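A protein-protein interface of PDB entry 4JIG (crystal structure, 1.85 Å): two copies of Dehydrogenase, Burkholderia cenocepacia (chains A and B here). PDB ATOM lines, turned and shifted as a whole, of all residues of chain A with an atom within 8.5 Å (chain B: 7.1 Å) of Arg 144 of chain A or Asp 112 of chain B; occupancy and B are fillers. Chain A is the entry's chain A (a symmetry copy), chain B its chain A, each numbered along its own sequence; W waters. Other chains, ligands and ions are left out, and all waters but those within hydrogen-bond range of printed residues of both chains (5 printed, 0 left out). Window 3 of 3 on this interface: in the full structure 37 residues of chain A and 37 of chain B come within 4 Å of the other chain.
The backbone NH (N) of Leu 110 of chain B is in hydrogen-bond range of the side-chain carboxylate (OE1) of Glu 187 of chain A.
O of Ala 111 of chain B lies within hydrogen-bond range of NE of Arg 138 of chain A.
The side-chain carboxylate (OD1) of Asp 112 of chain B lies within salt-bridge range of the guanidinium group (NH1) of Arg 144 of chain A (2.9 Å).
The guanidinium group of Arg 134 of chain A sits at hydrogen-bond distance from the backbone carbonyl oxygen of Met 113 of chain B (2.8 Å).
OE2 of Glu 187 of chain A sits at hydrogen-bond distance from N of Asn 165 of chain B (2.7 Å).
The side-chain sulfur of Met 113 of chain B is in hydrogen-bond range of the guanidinium group of Arg 117 of chain B (3.6 Å).
OE2 of Glu 135 of chain A is in salt-bridge range of NH1 of Arg 138 of chain A (3.8 Å).
Arg 134 of chain A touches Leu 110 of chain B.
Arg 134 of chain A touches Ala 111 of chain B.
Pro 114 of chain B touches Arg 134 of chain A.
Arg 134 of chain A touches Val 115 of chain B (NH2 to N, 3.5 Å).
Arg 138 of chain A touches Met 113 of chain B (NH2 to O, 3.9 Å).
CB of Ala 111 of chain B touches CZ of Arg 144 of chain A, 3.4 Å away.
Glu 187 of chain A touches Pro 109 of chain B (OE1 to CA, 3.5 Å).
Of chain B, only Ala 111 and Asp 112 come within 4 Å of Arg 144 of chain A.
Printed residues of chain B within 4 Å of Glu 187 of chain A: Pro 109 (3.5 Å), Leu 110 (2.7 Å) and Asn 165 (2.7 Å).
Of the printed residues of chain A, Leu 110 of chain B touches Arg 134 (3.5 Å) and Glu 187 (2.7 Å).
Asp 112 of chain B touches one residue of chain A.
Of the printed residues of chain A, Pro 114 of chain B touches Arg 134.
Of the printed residues of chain A, Asn 165 of chain B touches Glu 187.
The nearest residue of chain B that does not touch Arg 144 of chain A is Pro 109 of chain B (4.1 Å).
The nearest residue of chain A that does not touch Asp 112 of chain B is Arg 138 of chain A (4.7 Å).
Of the 18 printed residues of chain A, 4 touch a printed residue of chain B.
Among the printed residues, 12 pairs touch across the chains.
No position is printed for both chains.
Water W4 lies within hydrogen-bond range of the side-chain amide nitrogen of Asn 165 of chain B (2.6 Å), the backbone carbonyl oxygen of Glu 187 of chain A (3.1 Å) and a ring nitrogen (NE2) of His 191 of chain A (3.3 Å).
Water W2 lies within hydrogen-bond range of O of Met 108 of chain B (2.7 Å) and OE2 of Glu 187 of chain A (2.8 Å).
Water W1 lies within hydrogen-bond range of the side-chain carboxylate of Glu 187 of chain A, the backbone NH of Ala 111 of chain B and the backbone NH of Leu 110 of chain B.
Water W3 lies within hydrogen-bond range of O of Glu 187 of chain A (2.8 Å) and OD1 of Asn 165 of chain B (3.0 Å).
Water W5 bridges the backbone NH of Val 115 of chain B and the guanidinium group of Arg 134 of chain A.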
ATOM      1  N   ARG A 134       0.203  18.782  23.459  1.00  0.00           N
ATOM      2  CA  ARG A 134       0.478  17.611  22.619  1.00  0.00           C
ATOM      3  C   ARG A 134       0.320  16.317  23.433  1.00  0.00           C
ATOM      4  O   ARG A 134      -0.246  15.309  22.962  1.00  0.00           O
ATOM      5  CB  ARG A 134       1.881  17.692  22.005  1.00  0.00           C
ATOM      6  CG  ARG A 134       2.203  16.490  21.122  1.00  0.00           C
ATOM      7  CD  ARG A 134       3.610  16.513  20.533  1.00  0.00           C
ATOM      8  NE  ARG A 134       4.552  16.162  21.578  1.00  0.00           N
ATOM      9  CZ  ARG A 134       5.814  15.795  21.424  1.00  0.00           C
ATOM     10  NH1 ARG A 134       6.520  15.526  22.522  1.00  0.00           N
ATOM     11  NH2 ARG A 134       6.373  15.689  20.220  1.00  0.00           N
ATOM     12  N   GLU A 135       0.862  16.334  24.643  1.00  0.00           N
ATOM     13  CA  GLU A 135       0.778  15.161  25.525  1.00  0.00           C
ATOM     14  C   GLU A 135      -0.662  14.917  25.925  1.00  0.00           C
ATOM     15  O   GLU A 135      -1.111  13.785  25.969  1.00  0.00           O
ATOM     16  CB  GLU A 135       1.692  15.337  26.764  1.00  0.00           C
ATOM     17  CG  GLU A 135       2.285  14.050  27.329  1.00  0.00           C
ATOM     18  CD  GLU A 135       2.985  13.159  26.301  1.00  0.00           C
ATOM     19  OE1 GLU A 135       2.833  11.944  26.436  1.00  0.00           O
ATOM     20  OE2 GLU A 135       3.662  13.650  25.388  1.00  0.00           O
ATOM     21  N   ALA A 136      -1.414  15.974  26.188  1.00  0.00           N
ATOM     22  CA  ALA A 136      -2.844  15.800  26.518  1.00  0.00           C
ATOM     23  C   ALA A 136      -3.604  15.256  25.315  1.00  0.00           C
ATOM     24  O   ALA A 136      -4.451  14.363  25.433  1.00  0.00           O
ATOM     25  CB  ALA A 136      -3.456  17.115  27.025  1.00  0.00           C
ATOM     26  N   ALA A 137      -3.261  15.755  24.141  1.00  0.00           N
ATOM     27  CA  ALA A 137      -3.834  15.233  22.939  1.00  0.00           C
ATOM     28  C   ALA A 137      -3.566  13.715  22.811  1.00  0.00           C
ATOM     29  O   ALA A 137      -4.481  12.932  22.512  1.00  0.00           O
ATOM     30  CB  ALA A 137      -3.276  15.954  21.764  1.00  0.00           C
ATOM     31  N   ARG A 138      -2.311  13.316  23.009  1.00  0.00           N
ATOM     32  CA  ARG A 138      -1.955  11.879  22.945  1.00  0.00           C
ATOM     33  C   ARG A 138      -2.701  11.023  23.960  1.00  0.00           C
ATOM     34  O   ARG A 138      -3.107   9.903  23.630  1.00  0.00           O
ATOM     35  CB  ARG A 138      -0.470  11.658  23.120  1.00  0.00           C
ATOM     36  CG  ARG A 138       0.311  12.222  21.973  1.00  0.00           C
ATOM     37  CD  ARG A 138       1.799  12.285  22.291  1.00  0.00           C
ATOM     38  NE  ARG A 138       2.523  12.608  21.055  1.00  0.00           N
ATOM     39  CZ  ARG A 138       3.847  12.642  20.914  1.00  0.00           C
ATOM     40  NH1 ARG A 138       4.640  12.408  21.938  1.00  0.00           N
ATOM     41  NH2 ARG A 138       4.369  12.942  19.739  1.00  0.00           N
ATOM     42  N   ARG A 139      -2.920  11.559  25.157  1.00  0.00           N
ATOM     43  CA  ARG A 139      -3.439  10.775  26.270  1.00  0.00           C
ATOM     44  C   ARG A 139      -4.927  10.893  26.522  1.00  0.00           C
ATOM     45  O   ARG A 139      -5.508   9.949  27.057  1.00  0.00           O
ATOM     46  CB  ARG A 139      -2.741  11.195  27.532  1.00  0.00           C
ATOM     47  CG  ARG A 139      -1.258  11.094  27.335  1.00  0.00           C
ATOM     48  CD  ARG A 139      -0.541  10.958  28.613  1.00  0.00           C
ATOM     49  NE  ARG A 139       0.883  10.891  28.300  1.00  0.00           N
ATOM     50  CZ  ARG A 139       1.770  10.212  29.000  1.00  0.00           C
ATOM     51  NH1 ARG A 139       1.389   9.488  30.050  1.00  0.00           N
ATOM     52  NH2 ARG A 139       3.049  10.269  28.638  1.00  0.00           N
ATOM     53  N   LEU A 140      -5.531  12.023  26.172  1.00  0.00           N
ATOM     54  CA  LEU A 140      -6.964  12.210  26.402  1.00  0.00           C
ATOM     55  C   LEU A 140      -7.832  11.850  25.204  1.00  0.00           C
ATOM     56  O   LEU A 140      -9.020  11.528  25.391  1.00  0.00           O
ATOM     57  CB  LEU A 140      -7.269  13.647  26.795  1.00  0.00           C
ATOM     58  CG  LEU A 140      -6.554  14.173  28.045  1.00  0.00           C
ATOM     59  CD1 LEU A 140      -6.905  15.652  28.223  1.00  0.00           C
ATOM     60  CD2 LEU A 140      -6.976  13.303  29.228  1.00  0.00           C
ATOM     61  N   SER A 141      -7.280  11.907  23.991  1.00  0.00           N
ATOM     62  CA  SER A 141      -8.091  11.711  22.799  1.00  0.00           C
ATOM     63  C   SER A 141      -8.654  10.281  22.728  1.00  0.00           C
ATOM     64  O   SER A 141      -7.934   9.297  22.947  1.00  0.00           O
ATOM     65  CB  SER A 141      -7.304  11.987  21.523  1.00  0.00           C
ATOM     66  OG  SER A 141      -6.853  13.331  21.400  1.00  0.00           O
ATOM     67  N   THR A 142      -9.923  10.179  22.391  1.00  0.00           N
ATOM     68  CA  THR A 142     -10.579   8.876  22.359  1.00  0.00           C
ATOM     69  C   THR A 142     -10.024   7.998  21.250  1.00  0.00           C
ATOM     70  O   THR A 142     -10.066   6.772  21.371  1.00  0.00           O
ATOM     71  CB  THR A 142     -12.097   9.009  22.217  1.00  0.00           C
ATOM     72  OG1 THR A 142     -12.420   9.812  21.080  1.00  0.00           O
ATOM     73  CG2 THR A 142     -12.654   9.640  23.456  1.00  0.00           C
ATOM     74  N   ASP A 143      -9.479   8.613  20.191  1.00  0.00           N
ATOM     75  CA  ASP A 143      -8.872   7.850  19.088  1.00  0.00           C
ATOM     76  C   ASP A 143      -7.453   7.360  19.367  1.00  0.00           C
ATOM     77  O   ASP A 143      -6.855   6.646  18.551  1.00  0.00           O
ATOM     78  CB  ASP A 143      -8.920   8.658  17.820  1.00  0.00           C
ATOM     79  CG  ASP A 143      -8.049   9.920  17.879  1.00  0.00           C
ATOM     80  OD1 ASP A 143      -7.958  10.603  18.945  1.00  0.00           O
ATOM     81  OD2 ASP A 143      -7.492  10.192  16.827  1.00  0.00           O
ATOM     82  N   ARG A 144      -6.903   7.755  20.510  1.00  0.00           N
ATOM     83  CA  ARG A 144      -5.590   7.334  20.944  1.00  0.00           C
ATOM     84  C   ARG A 144      -5.691   6.576  22.289  1.00  0.00           C
ATOM     85  O   ARG A 144      -4.731   6.521  23.020  1.00  0.00           O
ATOM     86  CB  ARG A 144      -4.645   8.565  20.996  1.00  0.00           C
ATOM     87  CG  ARG A 144      -4.447   9.170  19.607  1.00  0.00           C
ATOM     88  CD  ARG A 144      -3.728  10.524  19.594  1.00  0.00           C
ATOM     89  NE  ARG A 144      -3.852  11.194  18.296  1.00  0.00           N
ATOM     90  CZ  ARG A 144      -2.963  11.165  17.297  1.00  0.00           C
ATOM     91  NH1 ARG A 144      -1.811  10.533  17.402  1.00  0.00           N
ATOM     92  NH2 ARG A 144      -3.203  11.855  16.202  1.00  0.00           N
ATOM     93  N   GLY A 145      -6.870   5.994  22.581  1.00  0.00           N
ATOM     94  CA  GLY A 145      -7.076   5.197  23.800  1.00  0.00           C
ATOM     95  C   GLY A 145      -7.553   5.922  25.063  1.00  0.00           C
ATOM     96  O   GLY A 145      -7.813   5.274  26.081  1.00  0.00           O
ATOM     97  N   GLY A 146      -7.696   7.249  25.022  1.00  0.00           N
ATOM     98  CA  GLY A 146      -8.060   8.020  26.221  1.00  0.00           C
ATOM     99  C   GLY A 146      -9.555   8.082  26.454  1.00  0.00           C
ATOM    100  O   GLY A 146     -10.375   7.642  25.622  1.00  0.00           O
ATOM    101  N   ARG A 147      -9.954   8.661  27.589  1.00  0.00           N
ATOM    102  CA  ARG A 147     -11.384   8.686  27.894  1.00  0.00           C
ATOM    103  C   ARG A 147     -12.055  10.025  27.609  1.00  0.00           C
ATOM    104  O   ARG A 147     -13.181  10.255  28.006  1.00  0.00           O
ATOM    105  CB  ARG A 147     -11.658   8.198  29.322  1.00  0.00           C
ATOM    106  CG  ARG A 147     -10.991   8.990  30.432  1.00  0.00           C
ATOM    107  CD  ARG A 147     -10.879   8.111  31.677  1.00  0.00           C
ATOM    108  NE  ARG A 147     -10.996   8.903  32.897  1.00  0.00           N
ATOM    109  CZ  ARG A 147     -11.344   8.404  34.075  1.00  0.00           C
ATOM    110  NH1 ARG A 147     -11.452   9.215  35.137  1.00  0.00           N
ATOM    111  NH2 ARG A 147     -11.627   7.107  34.182  1.00  0.00           N
ATOM    112  N   GLY A 148     -11.384  10.891  26.865  1.00  0.00           N
ATOM    113  CA  GLY A 148     -11.892  12.240  26.671  1.00  0.00           C
ATOM    114  C   GLY A 148     -11.475  13.159  27.809  1.00  0.00           C
ATOM    115  O   GLY A 148     -10.929  12.745  28.825  1.00  0.00           O
ATOM    116  N   GLU A 187      -9.363  20.478  16.150  1.00  0.00           N
ATOM    117  CA  GLU A 187      -8.669  19.246  15.926  1.00  0.00           C
ATOM    118  C   GLU A 187      -9.127  18.104  16.852  1.00  0.00           C
ATOM    119  O   GLU A 187      -9.278  16.961  16.414  1.00  0.00           O
ATOM    120  CB  GLU A 187      -7.173  19.551  16.119  1.00  0.00           C
ATOM    121  CG  GLU A 187      -6.231  18.501  15.651  1.00  0.00           C
ATOM    122  CD  GLU A 187      -4.800  19.005  15.592  1.00  0.00           C
ATOM    123  OE1 GLU A 187      -4.024  18.645  16.529  1.00  0.00           O
ATOM    124  OE2 GLU A 187      -4.479  19.750  14.654  1.00  0.00           O
ATOM    125  N   LEU A 188      -9.347  18.409  18.116  1.00  0.00           N
ATOM    126  CA  LEU A 188      -9.678  17.398  19.116  1.00  0.00           C
ATOM    127  C   LEU A 188     -11.161  17.215  19.434  1.00  0.00           C
ATOM    128  O   LEU A 188     -11.528  16.247  20.158  1.00  0.00           O
ATOM    129  CB  LEU A 188      -8.911  17.689  20.424  1.00  0.00           C
ATOM    130  CG  LEU A 188      -7.387  17.704  20.372  1.00  0.00           C
ATOM    131  CD1 LEU A 188      -6.817  17.816  21.789  1.00  0.00           C
ATOM    132  CD2 LEU A 188      -6.884  16.466  19.613  1.00  0.00           C
ATOM    133  N   HIS A 191     -12.599  13.858  18.894  1.00  0.00           N
ATOM    134  CA  HIS A 191     -11.979  12.869  19.773  1.00  0.00           C
ATOM    135  C   HIS A 191     -12.226  13.088  21.267  1.00  0.00           C
ATOM    136  O   HIS A 191     -11.485  12.607  22.105  1.00  0.00           O
ATOM    137  CB  HIS A 191     -10.481  12.845  19.487  1.00  0.00           C
ATOM    138  CG  HIS A 191     -10.171  12.801  18.029  1.00  0.00           C
ATOM    139  ND1 HIS A 191     -10.728  11.860  17.182  1.00  0.00           N
ATOM    140  CD2 HIS A 191      -9.380  13.587  17.258  1.00  0.00           C
ATOM    141  CE1 HIS A 191     -10.297  12.076  15.953  1.00  0.00           C
ATOM    142  NE2 HIS A 191      -9.479  13.114  15.973  1.00  0.00           N
ATOM    143  N   MET B 108      -0.216  17.620   9.659  1.00  0.00           N
ATOM    144  CA  MET B 108      -0.613  16.596  10.624  1.00  0.00           C
ATOM    145  C   MET B 108      -1.212  17.235  11.874  1.00  0.00           C
ATOM    146  O   MET B 108      -1.002  18.452  12.106  1.00  0.00           O
ATOM    147  CB  MET B 108       0.584  15.715  11.036  1.00  0.00           C
ATOM    148  CG  MET B 108       1.688  16.415  11.804  1.00  0.00           C
ATOM    149  SD  MET B 108       3.253  15.516  12.007  1.00  0.00           S
ATOM    150  CE  MET B 108       3.849  15.698  10.341  1.00  0.00           C
ATOM    151  N   PRO B 109      -1.923  16.460  12.678  1.00  0.00           N
ATOM    152  CA  PRO B 109      -2.378  16.901  13.999  1.00  0.00           C
ATOM    153  C   PRO B 109      -1.224  17.121  14.974  1.00  0.00           C
ATOM    154  O   PRO B 109      -0.137  16.540  14.815  1.00  0.00           O
ATOM    155  CB  PRO B 109      -3.261  15.755  14.502  1.00  0.00           C
ATOM    156  CG  PRO B 109      -3.386  14.809  13.371  1.00  0.00           C
ATOM    157  CD  PRO B 109      -2.325  15.070  12.391  1.00  0.00           C
ATOM    158  N   LEU B 110      -1.465  17.951  15.982  1.00  0.00           N
ATOM    159  CA  LEU B 110      -0.420  18.221  16.954  1.00  0.00           C
ATOM    160  C   LEU B 110       0.153  16.926  17.581  1.00  0.00           C
ATOM    161  O   LEU B 110       1.370  16.784  17.757  1.00  0.00           O
ATOM    162  CB  LEU B 110      -0.963  19.123  18.042  1.00  0.00           C
ATOM    163  CG  LEU B 110       0.005  19.438  19.187  1.00  0.00           C
ATOM    164  CD1 LEU B 110       1.281  20.107  18.692  1.00  0.00           C
ATOM    165  CD2 LEU B 110      -0.668  20.271  20.252  1.00  0.00           C
ATOM    166  N   ALA B 111      -0.729  16.011  17.934  1.00  0.00           N
ATOM    167  CA  ALA B 111      -0.318  14.768  18.568  1.00  0.00           C
ATOM    168  C   ALA B 111       0.814  14.009  17.832  1.00  0.00           C
ATOM    169  O   ALA B 111       1.590  13.301  18.482  1.00  0.00           O
ATOM    170  CB  ALA B 111      -1.521  13.844  18.719  1.00  0.00           C
ATOM    171  N   ASP B 112       0.856  14.123  16.507  1.00  0.00           N
ATOM    172  CA  ASP B 112       1.890  13.475  15.693  1.00  0.00           C
ATOM    173  C   ASP B 112       3.142  14.286  15.444  1.00  0.00           C
ATOM    174  O   ASP B 112       4.089  13.778  14.855  1.00  0.00           O
ATOM    175  CB  ASP B 112       1.253  13.080  14.366  1.00  0.00           C
ATOM    176  CG  ASP B 112       0.094  12.129  14.574  1.00  0.00           C
ATOM    177  OD1 ASP B 112       0.209  11.284  15.448  1.00  0.00           O
ATOM    178  OD2 ASP B 112      -0.937  12.278  13.933  1.00  0.00           O
ATOM    179  N   MET B 113       3.200  15.546  15.888  1.00  0.00           N
ATOM    180  CA  MET B 113       4.316  16.387  15.499  1.00  0.00           C
ATOM    181  C   MET B 113       5.506  16.107  16.385  1.00  0.00           C
ATOM    182  O   MET B 113       5.362  16.063  17.594  1.00  0.00           O
ATOM    183  CB  MET B 113       3.981  17.890  15.606  1.00  0.00           C
ATOM    184  CG  MET B 113       2.884  18.345  14.682  1.00  0.00           C
ATOM    185  SD  MET B 113       2.522  20.094  14.946  1.00  0.00           S
ATOM    186  CE  MET B 113       1.153  20.281  13.822  1.00  0.00           C
ATOM    187  N   PRO B 114       6.688  15.934  15.787  1.00  0.00           N
ATOM    188  CA  PRO B 114       7.848  15.736  16.635  1.00  0.00           C
ATOM    189  C   PRO B 114       8.340  17.050  17.165  1.00  0.00           C
ATOM    190  O   PRO B 114       8.134  18.107  16.537  1.00  0.00           O
ATOM    191  CB  PRO B 114       8.889  15.122  15.705  1.00  0.00           C
ATOM    192  CG  PRO B 114       8.475  15.547  14.347  1.00  0.00           C
ATOM    193  CD  PRO B 114       7.016  15.899  14.363  1.00  0.00           C
ATOM    194  N   VAL B 115       9.020  16.967  18.293  1.00  0.00           N
ATOM    195  CA  VAL B 115       9.522  18.139  18.952  1.00  0.00           C
ATOM    196  C   VAL B 115      10.485  18.970  18.107  1.00  0.00           C
ATOM    197  O   VAL B 115      10.472  20.185  18.197  1.00  0.00           O
ATOM    198  CB  VAL B 115      10.148  17.802  20.324  1.00  0.00           C
ATOM    199  CG1 VAL B 115      11.430  16.960  20.219  1.00  0.00           C
ATOM    200  CG2 VAL B 115      10.431  19.095  21.052  1.00  0.00           C
ATOM    201  N   ARG B 117      10.370  19.511  14.910  1.00  0.00           N
ATOM    202  CA  ARG B 117       9.550  20.325  14.016  1.00  0.00           C
ATOM    203  C   ARG B 117       8.941  21.528  14.782  1.00  0.00           C
ATOM    204  O   ARG B 117       8.917  22.650  14.268  1.00  0.00           O
ATOM    205  CB  ARG B 117       8.458  19.467  13.384  1.00  0.00           C
ATOM    206  CG  ARG B 117       7.449  20.211  12.548  1.00  0.00           C
ATOM    207  CD  ARG B 117       6.089  20.139  13.189  1.00  0.00           C
ATOM    208  NE  ARG B 117       5.028  20.936  12.557  1.00  0.00           N
ATOM    209  CZ  ARG B 117       4.228  20.512  11.579  1.00  0.00           C
ATOM    210  NH1 ARG B 117       4.404  19.304  11.035  1.00  0.00           N
ATOM    211  NH2 ARG B 117       3.235  21.299  11.138  1.00  0.00           N
ATOM    212  N   ASN B 165      -5.550  19.840  12.186  1.00  0.00           N
ATOM    213  CA  ASN B 165      -5.084  18.681  11.423  1.00  0.00           C
ATOM    214  C   ASN B 165      -4.076  18.969  10.381  1.00  0.00           C
ATOM    215  O   ASN B 165      -3.796  18.108   9.563  1.00  0.00           O
ATOM    216  CB  ASN B 165      -6.257  17.870  10.829  1.00  0.00           C
ATOM    217  CG  ASN B 165      -7.181  17.390  11.899  1.00  0.00           C
ATOM    218  OD1 ASN B 165      -8.370  17.661  11.867  1.00  0.00           O
ATOM    219  ND2 ASN B 165      -6.619  16.758  12.917  1.00  0.00           N
HETATM  220  O   HOH W   1      -3.527  16.406  18.071  1.00  0.00           O
HETATM  221  O   HOH W   2      -2.236  20.607  13.278  1.00  0.00           O
HETATM  222  O   HOH W   3     -10.347  16.443  13.825  1.00  0.00           O
HETATM  223  O   HOH W   4      -7.182  15.221  14.976  1.00  0.00           O
HETATM  224  O   HOH W   5       9.123  14.284  19.510  1.00  0.00           O
